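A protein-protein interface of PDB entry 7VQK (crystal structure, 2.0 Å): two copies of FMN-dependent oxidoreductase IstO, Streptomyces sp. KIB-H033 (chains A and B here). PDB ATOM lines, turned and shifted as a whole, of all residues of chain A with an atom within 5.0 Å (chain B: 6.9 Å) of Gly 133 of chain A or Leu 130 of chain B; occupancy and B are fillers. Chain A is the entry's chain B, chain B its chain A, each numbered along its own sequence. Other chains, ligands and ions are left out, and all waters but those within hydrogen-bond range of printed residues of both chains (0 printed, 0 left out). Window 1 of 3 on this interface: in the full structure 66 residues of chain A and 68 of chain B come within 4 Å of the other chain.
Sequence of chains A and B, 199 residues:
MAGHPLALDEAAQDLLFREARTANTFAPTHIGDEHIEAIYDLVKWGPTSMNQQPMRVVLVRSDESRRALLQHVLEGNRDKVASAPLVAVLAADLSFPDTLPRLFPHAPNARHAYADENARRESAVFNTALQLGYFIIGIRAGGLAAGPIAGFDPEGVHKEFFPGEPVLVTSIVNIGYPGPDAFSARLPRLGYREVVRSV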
ATOM      1  N   ALA A 129       5.033  24.341 -19.621  1.00  0.00           N
ATOM      2  CA  ALA A 129       6.280  23.955 -20.275  1.00  0.00           C
ATOM      3  C   ALA A 129       6.587  22.487 -20.017  1.00  0.00           C
ATOM      4  O   ALA A 129       6.994  21.755 -20.926  1.00  0.00           O
ATOM      5  CB  ALA A 129       7.416  24.848 -19.780  1.00  0.00           C
ATOM      6  N   LEU A 130       6.402  22.045 -18.773  1.00  0.00           N
ATOM      7  CA  LEU A 130       6.475  20.626 -18.456  1.00  0.00           C
ATOM      8  C   LEU A 130       5.600  19.808 -19.400  1.00  0.00           C
ATOM      9  O   LEU A 130       6.042  18.802 -19.975  1.00  0.00           O
ATOM     10  CB  LEU A 130       6.037  20.433 -17.005  1.00  0.00           C
ATOM     11  CG  LEU A 130       6.375  19.202 -16.202  1.00  0.00           C
ATOM     12  CD1 LEU A 130       7.878  18.909 -16.283  1.00  0.00           C
ATOM     13  CD2 LEU A 130       5.933  19.480 -14.781  1.00  0.00           C
ATOM     14  N   GLN A 131       4.346  20.228 -19.571  1.00  0.00           N
ATOM     15  CA  GLN A 131       3.434  19.504 -20.446  1.00  0.00           C
ATOM     16  C   GLN A 131       3.875  19.572 -21.899  1.00  0.00           C
ATOM     17  O   GLN A 131       3.594  18.650 -22.674  1.00  0.00           O
ATOM     18  CB  GLN A 131       2.012  20.062 -20.305  1.00  0.00           C
ATOM     19  CG  GLN A 131       1.388  19.798 -18.928  1.00  0.00           C
ATOM     20  CD  GLN A 131      -0.076  20.166 -18.885  1.00  0.00           C
ATOM     21  OE1 GLN A 131      -0.447  21.257 -18.453  1.00  0.00           O
ATOM     22  NE2 GLN A 131      -0.917  19.259 -19.349  1.00  0.00           N
ATOM     23  N   LEU A 132       4.529  20.660 -22.298  1.00  0.00           N
ATOM     24  CA  LEU A 132       5.062  20.721 -23.656  1.00  0.00           C
ATOM     25  C   LEU A 132       6.128  19.652 -23.849  1.00  0.00           C
ATOM     26  O   LEU A 132       6.222  19.040 -24.921  1.00  0.00           O
ATOM     27  CB  LEU A 132       5.631  22.111 -23.949  1.00  0.00           C
ATOM     28  CG  LEU A 132       6.443  22.181 -25.253  1.00  0.00           C
ATOM     29  CD1 LEU A 132       5.507  22.061 -26.460  1.00  0.00           C
ATOM     30  CD2 LEU A 132       7.266  23.471 -25.334  1.00  0.00           C
ATOM     31  N   GLY A 133       6.923  19.400 -22.808  1.00  0.00           N
ATOM     32  CA  GLY A 133       7.877  18.305 -22.869  1.00  0.00           C
ATOM     33  C   GLY A 133       7.194  16.975 -23.109  1.00  0.00           C
ATOM     34  O   GLY A 133       7.589  16.210 -23.993  1.00  0.00           O
ATOM     35  N   TYR A 134       6.146  16.686 -22.323  1.00  0.00           N
ATOM     36  CA  TYR A 134       5.351  15.483 -22.537  1.00  0.00           C
ATOM     37  C   TYR A 134       4.770  15.451 -23.948  1.00  0.00           C
ATOM     38  O   TYR A 134       4.783  14.411 -24.619  1.00  0.00           O
ATOM     39  CB  TYR A 134       4.222  15.403 -21.503  1.00  0.00           C
ATOM     40  CG  TYR A 134       4.645  15.497 -20.051  1.00  0.00           C
ATOM     41  CD1 TYR A 134       5.858  14.969 -19.617  1.00  0.00           C
ATOM     42  CD2 TYR A 134       3.811  16.101 -19.107  1.00  0.00           C
ATOM     43  CE1 TYR A 134       6.240  15.055 -18.269  1.00  0.00           C
ATOM     44  CE2 TYR A 134       4.178  16.192 -17.773  1.00  0.00           C
ATOM     45  CZ  TYR A 134       5.387  15.666 -17.354  1.00  0.00           C
ATOM     46  OH  TYR A 134       5.754  15.756 -16.022  1.00  0.00           O
ATOM     47  N   PHE A 135       4.221  16.581 -24.393  1.00  0.00           N
ATOM     48  CA  PHE A 135       3.566  16.645 -25.692  1.00  0.00           C
ATOM     49  C   PHE A 135       4.542  16.337 -26.820  1.00  0.00           C
ATOM     50  O   PHE A 135       4.217  15.591 -27.750  1.00  0.00           O
ATOM     51  CB  PHE A 135       2.951  18.029 -25.875  1.00  0.00           C
ATOM     52  CG  PHE A 135       2.033  18.148 -27.068  1.00  0.00           C
ATOM     53  CD1 PHE A 135       1.061  17.188 -27.332  1.00  0.00           C
ATOM     54  CD2 PHE A 135       2.106  19.253 -27.887  1.00  0.00           C
ATOM     55  CE1 PHE A 135       0.201  17.330 -28.421  1.00  0.00           C
ATOM     56  CE2 PHE A 135       1.259  19.395 -28.984  1.00  0.00           C
ATOM     57  CZ  PHE A 135       0.311  18.428 -29.244  1.00  0.00           C
ATOM     58  N   ILE A 136       5.749  16.892 -26.751  1.00  0.00           N
ATOM     59  CA  ILE A 136       6.740  16.592 -27.780  1.00  0.00           C
ATOM     60  C   ILE A 136       6.999  15.094 -27.837  1.00  0.00           C
ATOM     61  O   ILE A 136       6.965  14.479 -28.911  1.00  0.00           O
ATOM     62  CB  ILE A 136       8.023  17.401 -27.532  1.00  0.00           C
ATOM     63  CG1 ILE A 136       7.734  18.873 -27.855  1.00  0.00           C
ATOM     64  CG2 ILE A 136       9.174  16.848 -28.374  1.00  0.00           C
ATOM     65  CD1 ILE A 136       8.739  19.852 -27.318  1.00  0.00           C
ATOM     66  N   ILE A 137       7.224  14.477 -26.673  1.00  0.00           N
ATOM     67  CA  ILE A 137       7.410  13.026 -26.622  1.00  0.00           C
ATOM     68  C   ILE A 137       6.172  12.314 -27.148  1.00  0.00           C
ATOM     69  O   ILE A 137       6.264  11.292 -27.845  1.00  0.00           O
ATOM     70  CB  ILE A 137       7.750  12.592 -25.182  1.00  0.00           C
ATOM     71  CG1 ILE A 137       8.997  13.323 -24.691  1.00  0.00           C
ATOM     72  CG2 ILE A 137       7.953  11.088 -25.103  1.00  0.00           C
ATOM     73  CD1 ILE A 137       9.275  13.098 -23.183  1.00  0.00           C
ATOM     74  N   PHE B  17       4.063   6.367 -19.061  1.00  0.00           N
ATOM     75  CA  PHE B  17       2.906   7.235 -18.853  1.00  0.00           C
ATOM     76  C   PHE B  17       1.722   6.537 -18.186  1.00  0.00           C
ATOM     77  O   PHE B  17       1.258   6.966 -17.125  1.00  0.00           O
ATOM     78  CB  PHE B  17       2.435   7.820 -20.197  1.00  0.00           C
ATOM     79  CG  PHE B  17       3.315   8.918 -20.736  1.00  0.00           C
ATOM     80  CD1 PHE B  17       3.265  10.203 -20.199  1.00  0.00           C
ATOM     81  CD2 PHE B  17       4.165   8.673 -21.818  1.00  0.00           C
ATOM     82  CE1 PHE B  17       4.074  11.228 -20.713  1.00  0.00           C
ATOM     83  CE2 PHE B  17       4.981   9.693 -22.347  1.00  0.00           C
ATOM     84  CZ  PHE B  17       4.941  10.969 -21.790  1.00  0.00           C
ATOM     85  N   PRO B  47      14.559  18.151 -27.106  1.00  0.00           N
ATOM     86  CA  PRO B  47      14.928  19.453 -27.676  1.00  0.00           C
ATOM     87  C   PRO B  47      14.631  20.616 -26.741  1.00  0.00           C
ATOM     88  O   PRO B  47      13.679  20.601 -25.952  1.00  0.00           O
ATOM     89  CB  PRO B  47      14.068  19.541 -28.945  1.00  0.00           C
ATOM     90  CG  PRO B  47      12.831  18.726 -28.603  1.00  0.00           C
ATOM     91  CD  PRO B  47      13.337  17.601 -27.718  1.00  0.00           C
ATOM     92  N   THR B  48      15.480  21.634 -26.840  1.00  0.00           N
ATOM     93  CA  THR B  48      15.242  22.916 -26.194  1.00  0.00           C
ATOM     94  C   THR B  48      15.464  24.034 -27.210  1.00  0.00           C
ATOM     95  O   THR B  48      16.167  23.862 -28.210  1.00  0.00           O
ATOM     96  CB  THR B  48      16.150  23.115 -24.965  1.00  0.00           C
ATOM     97  OG1 THR B  48      17.507  22.810 -25.303  1.00  0.00           O
ATOM     98  CG2 THR B  48      15.723  22.192 -23.816  1.00  0.00           C
ATOM     99  N   SER B  49      14.861  25.191 -26.930  1.00  0.00           N
ATOM    100  CA  SER B  49      14.977  26.384 -27.766  1.00  0.00           C
ATOM    101  C   SER B  49      16.434  26.742 -28.037  1.00  0.00           C
ATOM    102  O   SER B  49      17.212  26.950 -27.103  1.00  0.00           O
ATOM    103  CB  SER B  49      14.269  27.551 -27.075  1.00  0.00           C
ATOM    104  OG  SER B  49      14.458  28.760 -27.785  1.00  0.00           O
ATOM    105  N   VAL B 125      14.212  29.248 -17.482  1.00  0.00           N
ATOM    106  CA  VAL B 125      13.285  28.464 -16.675  1.00  0.00           C
ATOM    107  C   VAL B 125      12.380  27.619 -17.558  1.00  0.00           C
ATOM    108  O   VAL B 125      12.144  26.437 -17.281  1.00  0.00           O
ATOM    109  CB  VAL B 125      12.479  29.402 -15.761  1.00  0.00           C
ATOM    110  CG1 VAL B 125      11.319  28.653 -15.101  1.00  0.00           C
ATOM    111  CG2 VAL B 125      13.408  30.006 -14.718  1.00  0.00           C
ATOM    112  N   PHE B 126      11.850  28.212 -18.629  1.00  0.00           N
ATOM    113  CA  PHE B 126      10.972  27.481 -19.529  1.00  0.00           C
ATOM    114  C   PHE B 126      11.666  26.245 -20.096  1.00  0.00           C
ATOM    115  O   PHE B 126      11.088  25.151 -20.121  1.00  0.00           O
ATOM    116  CB  PHE B 126      10.497  28.402 -20.658  1.00  0.00           C
ATOM    117  CG  PHE B 126       9.508  27.751 -21.576  1.00  0.00           C
ATOM    118  CD1 PHE B 126       9.939  27.050 -22.692  1.00  0.00           C
ATOM    119  CD2 PHE B 126       8.153  27.830 -21.316  1.00  0.00           C
ATOM    120  CE1 PHE B 126       9.041  26.428 -23.527  1.00  0.00           C
ATOM    121  CE2 PHE B 126       7.241  27.217 -22.156  1.00  0.00           C
ATOM    122  CZ  PHE B 126       7.689  26.519 -23.268  1.00  0.00           C
ATOM    123  N   ASN B 127      12.910  26.390 -20.567  1.00  0.00           N
ATOM    124  CA  ASN B 127      13.570  25.223 -21.151  1.00  0.00           C
ATOM    125  C   ASN B 127      14.054  24.237 -20.086  1.00  0.00           C
ATOM    126  O   ASN B 127      14.139  23.033 -20.360  1.00  0.00           O
ATOM    127  CB  ASN B 127      14.710  25.669 -22.073  1.00  0.00           C
ATOM    128  CG  ASN B 127      14.179  26.294 -23.365  1.00  0.00           C
ATOM    129  OD1 ASN B 127      13.863  25.590 -24.323  1.00  0.00           O
ATOM    130  ND2 ASN B 127      14.021  27.613 -23.362  1.00  0.00           N
ATOM    131  N   THR B 128      14.355  24.708 -18.875  1.00  0.00           N
ATOM    132  CA  THR B 128      14.660  23.774 -17.791  1.00  0.00           C
ATOM    133  C   THR B 128      13.414  23.000 -17.380  1.00  0.00           C
ATOM    134  O   THR B 128      13.515  21.840 -16.961  1.00  0.00           O
ATOM    135  CB  THR B 128      15.257  24.523 -16.595  1.00  0.00           C
ATOM    136  OG1 THR B 128      16.493  25.131 -16.988  1.00  0.00           O
ATOM    137  CG2 THR B 128      15.528  23.580 -15.416  1.00  0.00           C
ATOM    138  N   ALA B 129      12.235  23.624 -17.509  1.00  0.00           N
ATOM    139  CA  ALA B 129      10.986  22.910 -17.267  1.00  0.00           C
ATOM    140  C   ALA B 129      10.742  21.863 -18.341  1.00  0.00           C
ATOM    141  O   ALA B 129      10.325  20.740 -18.033  1.00  0.00           O
ATOM    142  CB  ALA B 129       9.814  23.895 -17.201  1.00  0.00           C
ATOM    143  N   LEU B 130      10.972  22.219 -19.611  1.00  0.00           N
ATOM    144  CA  LEU B 130      10.966  21.222 -20.675  1.00  0.00           C
ATOM    145  C   LEU B 130      11.859  20.048 -20.319  1.00  0.00           C
ATOM    146  O   LEU B 130      11.471  18.882 -20.454  1.00  0.00           O
ATOM    147  CB  LEU B 130      11.460  21.839 -21.981  1.00  0.00           C
ATOM    148  CG  LEU B 130      10.510  22.515 -22.951  1.00  0.00           C
ATOM    149  CD1 LEU B 130      11.281  22.824 -24.227  1.00  0.00           C
ATOM    150  CD2 LEU B 130       9.304  21.629 -23.231  1.00  0.00           C
ATOM    151  N   GLN B 131      13.096  20.346 -19.928  1.00  0.00           N
ATOM    152  CA  GLN B 131      14.043  19.290 -19.601  1.00  0.00           C
ATOM    153  C   GLN B 131      13.597  18.487 -18.385  1.00  0.00           C
ATOM    154  O   GLN B 131      13.868  17.281 -18.305  1.00  0.00           O
ATOM    155  CB  GLN B 131      15.423  19.896 -19.378  1.00  0.00           C
ATOM    156  CG  GLN B 131      16.020  20.516 -20.646  1.00  0.00           C
ATOM    157  CD  GLN B 131      17.458  20.879 -20.437  1.00  0.00           C
ATOM    158  OE1 GLN B 131      17.783  22.026 -20.137  1.00  0.00           O
ATOM    159  NE2 GLN B 131      18.335  19.887 -20.539  1.00  0.00           N
ATOM    160  N   LEU B 132      12.911  19.125 -17.433  1.00  0.00           N
ATOM    161  CA  LEU B 132      12.384  18.369 -16.300  1.00  0.00           C
ATOM    162  C   LEU B 132      11.373  17.337 -16.775  1.00  0.00           C
ATOM    163  O   LEU B 132      11.347  16.202 -16.285  1.00  0.00           O
ATOM    164  CB  LEU B 132      11.750  19.314 -15.275  1.00  0.00           C
ATOM    165  CG  LEU B 132      10.878  18.666 -14.172  1.00  0.00           C
ATOM    166  CD1 LEU B 132      11.668  17.661 -13.340  1.00  0.00           C
ATOM    167  CD2 LEU B 132      10.271  19.723 -13.274  1.00  0.00           C
ATOM    168  N   GLY B 133      10.522  17.719 -17.730  1.00  0.00           N
ATOM    169  CA  GLY B 133       9.587  16.758 -18.289  1.00  0.00           C
ATOM    170  C   GLY B 133      10.293  15.593 -18.955  1.00  0.00           C
ATOM    171  O   GLY B 133       9.897  14.435 -18.788  1.00  0.00           O
ATOM    172  N   TYR B 134      11.329  15.886 -19.750  1.00  0.00           N
ATOM    173  CA  TYR B 134      12.146  14.809 -20.302  1.00  0.00           C
ATOM    174  C   TYR B 134      12.771  13.985 -19.188  1.00  0.00           C
ATOM    175  O   TYR B 134      12.848  12.758 -19.282  1.00  0.00           O
ATOM    176  CB  TYR B 134      13.258  15.355 -21.195  1.00  0.00           C
ATOM    177  CG  TYR B 134      12.816  16.284 -22.305  1.00  0.00           C
ATOM    178  CD1 TYR B 134      11.572  16.143 -22.910  1.00  0.00           C
ATOM    179  CD2 TYR B 134      13.659  17.299 -22.753  1.00  0.00           C
ATOM    180  CE1 TYR B 134      11.168  17.003 -23.936  1.00  0.00           C
ATOM    181  CE2 TYR B 134      13.267  18.161 -23.777  1.00  0.00           C
ATOM    182  CZ  TYR B 134      12.025  18.005 -24.361  1.00  0.00           C
ATOM    183  OH  TYR B 134      11.639  18.859 -25.364  1.00  0.00           O
ATOM    184  N   PHE B 135      13.244  14.653 -18.135  1.00  0.00           N
ATOM    185  CA  PHE B 135      13.958  13.953 -17.070  1.00  0.00           C
ATOM    186  C   PHE B 135      13.023  13.020 -16.316  1.00  0.00           C
ATOM    187  O   PHE B 135      13.399  11.892 -15.968  1.00  0.00           O
ATOM    188  CB  PHE B 135      14.596  14.979 -16.131  1.00  0.00           C
ATOM    189  CG  PHE B 135      15.497  14.391 -15.065  1.00  0.00           C
ATOM    190  CD1 PHE B 135      16.498  13.481 -15.389  1.00  0.00           C
ATOM    191  CD2 PHE B 135      15.371  14.798 -13.753  1.00  0.00           C
ATOM    192  CE1 PHE B 135      17.321  12.957 -14.414  1.00  0.00           C
ATOM    193  CE2 PHE B 135      16.210  14.272 -12.750  1.00  0.00           C
ATOM    194  CZ  PHE B 135      17.186  13.359 -13.090  1.00  0.00           C
ATOM    195  N   ILE B 137      10.376  11.530 -17.587  1.00  0.00           N
ATOM    196  CA  ILE B 137      10.214  10.378 -18.472  1.00  0.00           C
ATOM    197  C   ILE B 137      11.468   9.506 -18.441  1.00  0.00           C
ATOM    198  O   ILE B 137      11.390   8.271 -18.456  1.00  0.00           O
ATOM    199  CB  ILE B 137       9.887  10.841 -19.907  1.00  0.00           C
ATOM    200  CG1 ILE B 137       8.634  11.729 -19.920  1.00  0.00           C
ATOM    201  CG2 ILE B 137       9.735   9.632 -20.839  1.00  0.00           C
ATOM    202  CD1 ILE B 137       7.591  11.322 -18.905  1.00  0.00           C
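The side-chain hydroxyl of Tyr 134 of chain B sits at hydrogen-bond distance from the backbone carbonyl oxygen of Pro 47 of chain B.
Among the printed residues, pairs that only touch across the chains: Ala 129 of chain A with Phe 126 of chain B (3.4 Å), Ala 129 of chain A with Ala 129 of chain B (3.6 Å), Ala 129 of chain A with Leu 130 of chain B (3.3 Å), Leu 130 of chain A with Ala 129 of chain B (3.5 Å), Leu 130 of chain A with Leu 132 of chain B (3.7 Å), Leu 130 of chain A with Gly 133 of chain B (3.2 Å), Leu 132 of chain A with Phe 126 of chain B (3.7 Å), Leu 132 of chain A with Leu 130 of chain B (3.5 Å), Gly 133 of chain A with Leu 130 of chain B (3.3 Å), Gly 133 of chain A with Tyr 134 of chain B (3.7 Å), Tyr 134 of chain A with Gly 133 of chain B (3.7 Å), Ile 136 of chain A with Tyr 134 of chain B (3.6 Å), Ile 137 of chain A with Tyr 134 of chain B (3.8 Å) and Ile 137 of chain A with Ile 137 of chain B (3.6 Å).
Of the printed residues of chain B, Leu 132 of chain A touches Phe 126 (3.7 Å) and Leu 130 (3.5 Å). Of chain B, only Leu 130 and Tyr 134 come within 4 Å of Gly 133 of chain A. Printed residues of chain B within 4 Å of Tyr 134 of chain A: Gly 133 (3.7 Å). Of the printed residues of chain A, Phe 126 of chain B touches Ala 129 and Leu 132. Of chain A, only Ala 129, Leu 132 and Gly 133 come within 4 Å of Leu 130 of chain B. Of the printed residues of chain A, Gly 133 of chain B touches Leu 130 (3.2 Å) and Tyr 134 (3.7 Å). Of the printed residues of chain A, Tyr 134 of chain B touches Gly 133 (3.7 Å), Ile 136 (3.6 Å) and Ile 137 (3.8 Å). The nearest residue of chain B that does not touch Gly 133 of chain A is Gly 133 of chain B (5.1 Å). The nearest residue of chain A that does not touch Leu 130 of chain B is Ile 136 of chain A (4.5 Å).
Hydrophobic or aromatic side chains of chain B within 4 Å of the printed part of chain A: Phe 126, Ala 129, Leu 130, Leu 132, Tyr 134 and Ile 137. Along chain B the printed residues that touch a printed residue of chain A span positions 126 to 137. Printed residues of chain A that touch a printed residue of chain B: Ala 129, Leu 130, Leu 132, Gly 133, Tyr 134, Ile 136 and Ile 137. Hydrophobic or aromatic side chains of chain A within 4 Å of the printed part of chain B: Ala 129, Leu 130, Leu 132, Tyr 134, Ile 136 and Ile 137.
Ala 129 of chain A touches its own counterpart, Ala 129 of chain B. Ala 129 of chain A touches Leu 130 of chain B, and with the chains exchanged Leu 130 of chain A touches Ala 129 of chain B. Leu 130 of chain A touches Gly 133 of chain B, and with the chains exchanged Gly 133 of chain A touches Leu 130 of chain B. Ile 137 of chain A touches Tyr 134 of chain B, but with the chains exchanged Tyr 134 of chain A does not touch Ile 137 of chain B (4.02 Å).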
